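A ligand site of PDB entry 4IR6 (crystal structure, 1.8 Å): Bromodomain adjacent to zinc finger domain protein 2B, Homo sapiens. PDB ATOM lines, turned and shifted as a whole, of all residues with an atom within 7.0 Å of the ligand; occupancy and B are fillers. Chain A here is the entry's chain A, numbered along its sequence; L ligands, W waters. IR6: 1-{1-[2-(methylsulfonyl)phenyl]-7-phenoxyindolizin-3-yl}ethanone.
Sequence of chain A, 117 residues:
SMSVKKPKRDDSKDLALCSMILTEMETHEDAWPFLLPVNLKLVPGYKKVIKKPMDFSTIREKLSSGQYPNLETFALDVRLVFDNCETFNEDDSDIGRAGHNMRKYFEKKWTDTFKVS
The side-chain amide nitrogen of Asn 89 is in hydrogen-bond range of the backbone carbonyl oxygen of Cys 85, at 3.0 Å.
OD1 of Asn 39 sits at hydrogen-bond distance from N of Leu 42, 3.3 Å away.
O of Ile 95 sits at hydrogen-bond distance from SG of Cys 85.
Water W6 lies within hydrogen-bond range of OH of Tyr 46 (2.6 Å), O01 of the ligand (3.0 Å), N of Cys 85 (3.3 Å) and O of Asn 84 (3.5 Å).
Merely in contact with the ligand: Trp 32 (3.7 Å), Pro 33 (3.2 Å), Phe 34 (3.8 Å), Leu 36 (3.1 Å), Pro 37 (3.4 Å), Val 38 (3.5 Å), Leu 42 (3.98 Å), Val 43 (3.4 Å) and Ile 95 (3.7 Å).
Of the 21 residues printed, 11 come within 4 Å of the ligand.
The side-chain amide nitrogen of Asn 89 is in hydrogen-bond range of an oxygen (O01) of the ligand, 3.1 Å away.
The backbone NH (N) of Asn 39 is in hydrogen-bond range of an oxygen (O03) of the ligand (3.2 Å).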
ATOM      1  N   TRP A  32      -6.932 -17.896  -6.958  1.00  0.00           N
ATOM      2  CA  TRP A  32      -7.664 -18.879  -7.753  1.00  0.00           C
ATOM      3  C   TRP A  32      -6.802 -19.739  -8.671  1.00  0.00           C
ATOM      4  O   TRP A  32      -7.142 -20.906  -8.847  1.00  0.00           O
ATOM      5  CB  TRP A  32      -8.852 -18.253  -8.526  1.00  0.00           C
ATOM      6  CG  TRP A  32      -8.476 -17.124  -9.423  1.00  0.00           C
ATOM      7  CD1 TRP A  32      -8.435 -15.801  -9.093  1.00  0.00           C
ATOM      8  CD2 TRP A  32      -8.028 -17.218 -10.767  1.00  0.00           C
ATOM      9  NE1 TRP A  32      -8.027 -15.059 -10.156  1.00  0.00           N
ATOM     10  CE2 TRP A  32      -7.729 -15.902 -11.201  1.00  0.00           C
ATOM     11  CE3 TRP A  32      -7.832 -18.289 -11.670  1.00  0.00           C
ATOM     12  CZ2 TRP A  32      -7.287 -15.619 -12.497  1.00  0.00           C
ATOM     13  CZ3 TRP A  32      -7.371 -18.003 -12.962  1.00  0.00           C
ATOM     14  CH2 TRP A  32      -7.109 -16.681 -13.364  1.00  0.00           C
ATOM     15  N   PRO A  33      -5.676 -19.222  -9.230  1.00  0.00           N
ATOM     16  CA  PRO A  33      -4.872 -20.132 -10.085  1.00  0.00           C
ATOM     17  C   PRO A  33      -4.057 -21.190  -9.276  1.00  0.00           C
ATOM     18  O   PRO A  33      -3.537 -22.124  -9.884  1.00  0.00           O
ATOM     19  CB  PRO A  33      -3.884 -19.195 -10.787  1.00  0.00           C
ATOM     20  CG  PRO A  33      -4.475 -17.791 -10.638  1.00  0.00           C
ATOM     21  CD  PRO A  33      -5.154 -17.809  -9.298  1.00  0.00           C
ATOM     22  N   PHE A  34      -3.997 -21.032  -7.946  1.00  0.00           N
ATOM     23  CA  PHE A  34      -3.012 -21.695  -7.105  1.00  0.00           C
ATOM     24  C   PHE A  34      -3.596 -22.615  -6.078  1.00  0.00           C
ATOM     25  O   PHE A  34      -2.859 -23.195  -5.286  1.00  0.00           O
ATOM     26  CB  PHE A  34      -2.090 -20.649  -6.430  1.00  0.00           C
ATOM     27  CG  PHE A  34      -1.558 -19.598  -7.387  1.00  0.00           C
ATOM     28  CD1 PHE A  34      -0.707 -19.964  -8.468  1.00  0.00           C
ATOM     29  CD2 PHE A  34      -1.953 -18.286  -7.283  1.00  0.00           C
ATOM     30  CE1 PHE A  34      -0.281 -19.025  -9.389  1.00  0.00           C
ATOM     31  CE2 PHE A  34      -1.518 -17.336  -8.204  1.00  0.00           C
ATOM     32  CZ  PHE A  34      -0.693 -17.698  -9.262  1.00  0.00           C
ATOM     33  N   LEU A  35      -4.908 -22.785  -6.088  1.00  0.00           N
ATOM     34  CA  LEU A  35      -5.601 -23.530  -5.038  1.00  0.00           C
ATOM     35  C   LEU A  35      -5.412 -25.015  -5.187  1.00  0.00           C
ATOM     36  O   LEU A  35      -5.405 -25.738  -4.200  1.00  0.00           O
ATOM     37  CB  LEU A  35      -7.083 -23.195  -4.988  1.00  0.00           C
ATOM     38  CG  LEU A  35      -7.416 -21.733  -4.623  1.00  0.00           C
ATOM     39  CD1 LEU A  35      -8.932 -21.501  -4.596  1.00  0.00           C
ATOM     40  CD2 LEU A  35      -6.744 -21.361  -3.353  1.00  0.00           C
ATOM     41  N   LEU A  36      -5.306 -25.489  -6.427  1.00  0.00           N
ATOM     42  CA  LEU A  36      -5.155 -26.915  -6.727  1.00  0.00           C
ATOM     43  C   LEU A  36      -3.965 -27.111  -7.657  1.00  0.00           C
ATOM     44  O   LEU A  36      -3.563 -26.201  -8.342  1.00  0.00           O
ATOM     45  CB  LEU A  36      -6.425 -27.399  -7.462  1.00  0.00           C
ATOM     46  CG  LEU A  36      -7.753 -27.294  -6.710  1.00  0.00           C
ATOM     47  CD1 LEU A  36      -8.957 -27.693  -7.568  1.00  0.00           C
ATOM     48  CD2 LEU A  36      -7.685 -28.180  -5.464  1.00  0.00           C
ATOM     49  N   PRO A  37      -3.418 -28.334  -7.705  1.00  0.00           N
ATOM     50  CA  PRO A  37      -2.423 -28.622  -8.731  1.00  0.00           C
ATOM     51  C   PRO A  37      -2.882 -28.252 -10.156  1.00  0.00           C
ATOM     52  O   PRO A  37      -4.038 -28.455 -10.513  1.00  0.00           O
ATOM     53  CB  PRO A  37      -2.242 -30.150  -8.659  1.00  0.00           C
ATOM     54  CG  PRO A  37      -2.947 -30.588  -7.437  1.00  0.00           C
ATOM     55  CD  PRO A  37      -3.828 -29.508  -6.921  1.00  0.00           C
ATOM     56  N   VAL A  38      -1.965 -27.750 -10.941  1.00  0.00           N
ATOM     57  CA  VAL A  38      -2.227 -27.487 -12.355  1.00  0.00           C
ATOM     58  C   VAL A  38      -2.635 -28.791 -12.968  1.00  0.00           C
ATOM     59  O   VAL A  38      -2.037 -29.844 -12.720  1.00  0.00           O
ATOM     60  CB  VAL A  38      -0.993 -26.866 -13.055  1.00  0.00           C
ATOM     61  CG1 VAL A  38      -1.196 -26.734 -14.579  1.00  0.00           C
ATOM     62  CG2 VAL A  38      -0.659 -25.547 -12.442  1.00  0.00           C
ATOM     63  N   ASN A  39      -3.737 -28.760 -13.692  1.00  0.00           N
ATOM     64  CA  ASN A  39      -4.342 -29.941 -14.224  1.00  0.00           C
ATOM     65  C   ASN A  39      -3.557 -30.516 -15.405  1.00  0.00           C
ATOM     66  O   ASN A  39      -3.605 -29.962 -16.537  1.00  0.00           O
ATOM     67  CB  ASN A  39      -5.766 -29.622 -14.655  1.00  0.00           C
ATOM     68  CG  ASN A  39      -6.576 -30.862 -14.901  1.00  0.00           C
ATOM     69  OD1 ASN A  39      -6.124 -31.826 -15.560  1.00  0.00           O
ATOM     70  ND2 ASN A  39      -7.793 -30.864 -14.371  1.00  0.00           N
ATOM     71  N   LEU A  40      -2.862 -31.621 -15.142  1.00  0.00           N
ATOM     72  CA  LEU A  40      -1.861 -32.084 -16.088  1.00  0.00           C
ATOM     73  C   LEU A  40      -2.477 -32.739 -17.303  1.00  0.00           C
ATOM     74  O   LEU A  40      -1.788 -32.993 -18.314  1.00  0.00           O
ATOM     75  CB  LEU A  40      -0.893 -33.058 -15.424  1.00  0.00           C
ATOM     76  CG  LEU A  40      -0.064 -32.529 -14.265  1.00  0.00           C
ATOM     77  CD1 LEU A  40       0.915 -33.611 -13.845  1.00  0.00           C
ATOM     78  CD2 LEU A  40       0.651 -31.230 -14.607  1.00  0.00           C
ATOM     79  N   LEU A  42      -5.267 -31.339 -18.731  1.00  0.00           N
ATOM     80  CA  LEU A  42      -5.918 -30.303 -19.474  1.00  0.00           C
ATOM     81  C   LEU A  42      -4.973 -29.191 -19.872  1.00  0.00           C
ATOM     82  O   LEU A  42      -5.357 -28.345 -20.694  1.00  0.00           O
ATOM     83  CB  LEU A  42      -7.072 -29.730 -18.656  1.00  0.00           C
ATOM     84  CG  LEU A  42      -8.267 -30.697 -18.493  1.00  0.00           C
ATOM     85  CD1 LEU A  42      -9.244 -30.190 -17.436  1.00  0.00           C
ATOM     86  CD2 LEU A  42      -8.981 -30.890 -19.820  1.00  0.00           C
ATOM     87  N   VAL A  43      -3.768 -29.134 -19.306  1.00  0.00           N
ATOM     88  CA  VAL A  43      -2.926 -27.991 -19.567  1.00  0.00           C
ATOM     89  C   VAL A  43      -1.744 -28.458 -20.385  1.00  0.00           C
ATOM     90  O   VAL A  43      -0.826 -29.057 -19.821  1.00  0.00           O
ATOM     91  CB  VAL A  43      -2.450 -27.272 -18.307  1.00  0.00           C
ATOM     92  CG1 VAL A  43      -1.632 -26.054 -18.699  1.00  0.00           C
ATOM     93  CG2 VAL A  43      -3.662 -26.816 -17.483  1.00  0.00           C
ATOM     94  N   PRO A  44      -1.808 -28.254 -21.726  1.00  0.00           N
ATOM     95  CA  PRO A  44      -0.696 -28.731 -22.601  1.00  0.00           C
ATOM     96  C   PRO A  44       0.650 -28.102 -22.183  1.00  0.00           C
ATOM     97  O   PRO A  44       0.678 -26.920 -21.798  1.00  0.00           O
ATOM     98  CB  PRO A  44      -1.137 -28.313 -24.044  1.00  0.00           C
ATOM     99  CG  PRO A  44      -2.512 -27.704 -23.935  1.00  0.00           C
ATOM    100  CD  PRO A  44      -2.904 -27.586 -22.478  1.00  0.00           C
ATOM    101  N   TYR A  46       2.482 -28.536 -19.474  1.00  0.00           N
ATOM    102  CA  TYR A  46       2.810 -28.272 -18.056  1.00  0.00           C
ATOM    103  C   TYR A  46       3.763 -29.287 -17.501  1.00  0.00           C
ATOM    104  O   TYR A  46       4.834 -28.954 -16.955  1.00  0.00           O
ATOM    105  CB  TYR A  46       1.565 -28.162 -17.159  1.00  0.00           C
ATOM    106  CG  TYR A  46       1.917 -27.326 -15.970  1.00  0.00           C
ATOM    107  CD1 TYR A  46       2.336 -27.900 -14.777  1.00  0.00           C
ATOM    108  CD2 TYR A  46       1.988 -25.928 -16.087  1.00  0.00           C
ATOM    109  CE1 TYR A  46       2.658 -27.109 -13.668  1.00  0.00           C
ATOM    110  CE2 TYR A  46       2.397 -25.137 -15.000  1.00  0.00           C
ATOM    111  CZ  TYR A  46       2.700 -25.724 -13.788  1.00  0.00           C
ATOM    112  OH  TYR A  46       3.118 -24.943 -12.739  1.00  0.00           O
ATOM    113  N   MET A  54       3.869 -27.189  -7.858  1.00  0.00           N
ATOM    114  CA  MET A  54       3.479 -26.937  -6.446  1.00  0.00           C
ATOM    115  C   MET A  54       2.259 -26.042  -6.470  1.00  0.00           C
ATOM    116  O   MET A  54       2.054 -25.241  -7.387  1.00  0.00           O
ATOM    117  CB  MET A  54       4.673 -26.348  -5.651  1.00  0.00           C
ATOM    118  CG  MET A  54       4.455 -26.224  -4.145  1.00  0.00           C
ATOM    119  SD  MET A  54       3.902 -27.720  -3.362  1.00  0.00           S
ATOM    120  CE  MET A  54       5.170 -28.856  -3.879  1.00  0.00           C
ATOM    121  N   ASP A  55       1.444 -26.142  -5.427  1.00  0.00           N
ATOM    122  CA  ASP A  55       0.238 -25.377  -5.287  1.00  0.00           C
ATOM    123  C   ASP A  55      -0.132 -25.285  -3.818  1.00  0.00           C
ATOM    124  O   ASP A  55       0.408 -26.049  -3.003  1.00  0.00           O
ATOM    125  CB  ASP A  55      -0.896 -26.041  -6.069  1.00  0.00           C
ATOM    126  CG  ASP A  55      -1.388 -27.313  -5.427  1.00  0.00           C
ATOM    127  OD1 ASP A  55      -2.469 -27.282  -4.778  1.00  0.00           O
ATOM    128  OD2 ASP A  55      -0.703 -28.344  -5.568  1.00  0.00           O
ATOM    129  N   VAL A  81       5.681 -22.072  -6.176  1.00  0.00           N
ATOM    130  CA  VAL A  81       4.407 -21.800  -6.813  1.00  0.00           C
ATOM    131  C   VAL A  81       4.552 -20.594  -7.784  1.00  0.00           C
ATOM    132  O   VAL A  81       4.148 -20.648  -8.957  1.00  0.00           O
ATOM    133  CB  VAL A  81       3.261 -21.516  -5.800  1.00  0.00           C
ATOM    134  CG1 VAL A  81       1.973 -21.146  -6.530  1.00  0.00           C
ATOM    135  CG2 VAL A  81       3.014 -22.714  -4.886  1.00  0.00           C
ATOM    136  N   ASN A  84       7.112 -21.135 -10.750  1.00  0.00           N
ATOM    137  CA  ASN A  84       6.491 -21.931 -11.801  1.00  0.00           C
ATOM    138  C   ASN A  84       5.488 -21.094 -12.607  1.00  0.00           C
ATOM    139  O   ASN A  84       5.455 -21.166 -13.826  1.00  0.00           O
ATOM    140  CB  ASN A  84       5.727 -23.097 -11.198  1.00  0.00           C
ATOM    141  CG  ASN A  84       6.622 -24.173 -10.620  1.00  0.00           C
ATOM    142  OD1 ASN A  84       7.858 -24.223 -10.856  1.00  0.00           O
ATOM    143  ND2 ASN A  84       6.022 -25.038  -9.802  1.00  0.00           N
ATOM    144  N   CYS A  85       4.715 -20.265 -11.904  1.00  0.00           N
ATOM    145  CA  CYS A  85       3.762 -19.385 -12.530  1.00  0.00           C
ATOM    146  C   CYS A  85       4.432 -18.470 -13.524  1.00  0.00           C
ATOM    147  O   CYS A  85       3.978 -18.351 -14.659  1.00  0.00           O
ATOM    148  CB  CYS A  85       2.944 -18.588 -11.479  1.00  0.00           C
ATOM    149  SG  CYS A  85       1.626 -17.602 -12.197  1.00  0.00           S
ATOM    150  N   PHE A  88       5.697 -20.310 -16.783  1.00  0.00           N
ATOM    151  CA  PHE A  88       4.673 -20.850 -17.635  1.00  0.00           C
ATOM    152  C   PHE A  88       3.730 -19.817 -18.203  1.00  0.00           C
ATOM    153  O   PHE A  88       3.163 -20.069 -19.257  1.00  0.00           O
ATOM    154  CB  PHE A  88       3.872 -21.952 -16.941  1.00  0.00           C
ATOM    155  CG  PHE A  88       3.236 -22.923 -17.907  1.00  0.00           C
ATOM    156  CD1 PHE A  88       3.992 -23.890 -18.546  1.00  0.00           C
ATOM    157  CD2 PHE A  88       1.887 -22.852 -18.201  1.00  0.00           C
ATOM    158  CE1 PHE A  88       3.427 -24.771 -19.466  1.00  0.00           C
ATOM    159  CE2 PHE A  88       1.321 -23.740 -19.109  1.00  0.00           C
ATOM    160  CZ  PHE A  88       2.086 -24.686 -19.751  1.00  0.00           C
ATOM    161  N   ASN A  89       3.587 -18.660 -17.565  1.00  0.00           N
ATOM    162  CA  ASN A  89       2.601 -17.680 -17.938  1.00  0.00           C
ATOM    163  C   ASN A  89       3.231 -16.318 -18.253  1.00  0.00           C
ATOM    164  O   ASN A  89       4.183 -15.897 -17.588  1.00  0.00           O
ATOM    165  CB  ASN A  89       1.605 -17.466 -16.808  1.00  0.00           C
ATOM    166  CG  ASN A  89       0.859 -18.719 -16.443  1.00  0.00           C
ATOM    167  OD1 ASN A  89      -0.186 -19.021 -17.034  1.00  0.00           O
ATOM    168  ND2 ASN A  89       1.361 -19.450 -15.464  1.00  0.00           N
ATOM    169  N   ILE A  95      -3.443 -14.965 -15.092  1.00  0.00           N
ATOM    170  CA  ILE A  95      -2.752 -15.840 -14.190  1.00  0.00           C
ATOM    171  C   ILE A  95      -1.373 -15.249 -13.808  1.00  0.00           C
ATOM    172  O   ILE A  95      -0.979 -15.305 -12.619  1.00  0.00           O
ATOM    173  CB  ILE A  95      -2.598 -17.276 -14.752  1.00  0.00           C
ATOM    174  CG1 ILE A  95      -3.970 -17.959 -14.907  1.00  0.00           C
ATOM    175  CG2 ILE A  95      -1.702 -18.112 -13.876  1.00  0.00           C
ATOM    176  CD1 ILE A  95      -3.932 -19.225 -15.722  1.00  0.00           C
HETATM  177  C01 IR6 L   1      -0.858 -21.721 -11.998  1.00  0.00           C
HETATM  178  C02 IR6 L   1      -1.054 -21.972 -13.516  1.00  0.00           C
HETATM  179  O01 IR6 L   1      -0.127 -21.865 -14.301  1.00  0.00           O
HETATM  180  C03 IR6 L   1      -2.337 -22.322 -13.917  1.00  0.00           C
HETATM  181  C04 IR6 L   1      -3.468 -22.374 -13.068  1.00  0.00           C
HETATM  182  C05 IR6 L   1      -4.577 -22.777 -13.891  1.00  0.00           C
HETATM  183  C06 IR6 L   1      -5.970 -22.859 -13.456  1.00  0.00           C
HETATM  184  C07 IR6 L   1      -6.665 -21.677 -13.665  1.00  0.00           C
HETATM  185  C08 IR6 L   1      -8.000 -21.593 -13.323  1.00  0.00           C
HETATM  186  C09 IR6 L   1      -8.624 -22.634 -12.677  1.00  0.00           C
HETATM  187  C10 IR6 L   1      -7.958 -23.799 -12.437  1.00  0.00           C
HETATM  188  C11 IR6 L   1      -6.618 -23.897 -12.795  1.00  0.00           C
HETATM  189  S   IR6 L   1      -5.835 -25.438 -12.439  1.00  0.00           S
HETATM  190  C12 IR6 L   1      -4.809 -25.158 -11.030  1.00  0.00           C
HETATM  191  O02 IR6 L   1      -6.862 -26.372 -12.055  1.00  0.00           O
HETATM  192  O03 IR6 L   1      -4.991 -25.781 -13.550  1.00  0.00           O
HETATM  193  C13 IR6 L   1      -4.090 -22.882 -15.212  1.00  0.00           C
HETATM  194  C14 IR6 L   1      -4.716 -23.208 -16.441  1.00  0.00           C
HETATM  195  C15 IR6 L   1      -3.961 -23.247 -17.557  1.00  0.00           C
HETATM  196  O1  IR6 L   1      -4.454 -23.565 -18.830  1.00  0.00           O
HETATM  197  C16 IR6 L   1      -5.828 -23.546 -19.117  1.00  0.00           C
HETATM  198  C17 IR6 L   1      -6.460 -24.751 -19.395  1.00  0.00           C
HETATM  199  C18 IR6 L   1      -7.817 -24.748 -19.705  1.00  0.00           C
HETATM  200  C19 IR6 L   1      -8.526 -23.562 -19.749  1.00  0.00           C
HETATM  201  C20 IR6 L   1      -7.876 -22.372 -19.494  1.00  0.00           C
HETATM  202  C21 IR6 L   1      -6.518 -22.348 -19.159  1.00  0.00           C
HETATM  203  C22 IR6 L   1      -2.600 -22.978 -17.540  1.00  0.00           C
HETATM  204  C1  IR6 L   1      -1.985 -22.675 -16.350  1.00  0.00           C
HETATM  205  N1  IR6 L   1      -2.705 -22.652 -15.190  1.00  0.00           N
HETATM  206  O   HOH W   1      -6.639 -23.685  -8.604  1.00  0.00           O
HETATM  207  O   HOH W   2      -8.047 -28.646 -11.620  1.00  0.00           O
HETATM  208  O   HOH W   3      -1.957 -24.287  -9.463  1.00  0.00           O
HETATM  209  O   HOH W   4     -11.021 -20.588 -11.224  1.00  0.00           O
HETATM  210  O   HOH W   5       2.107 -21.908 -10.221  1.00  0.00           O
HETATM  211  O   HOH W   6       2.385 -22.462 -12.873  1.00  0.00           O
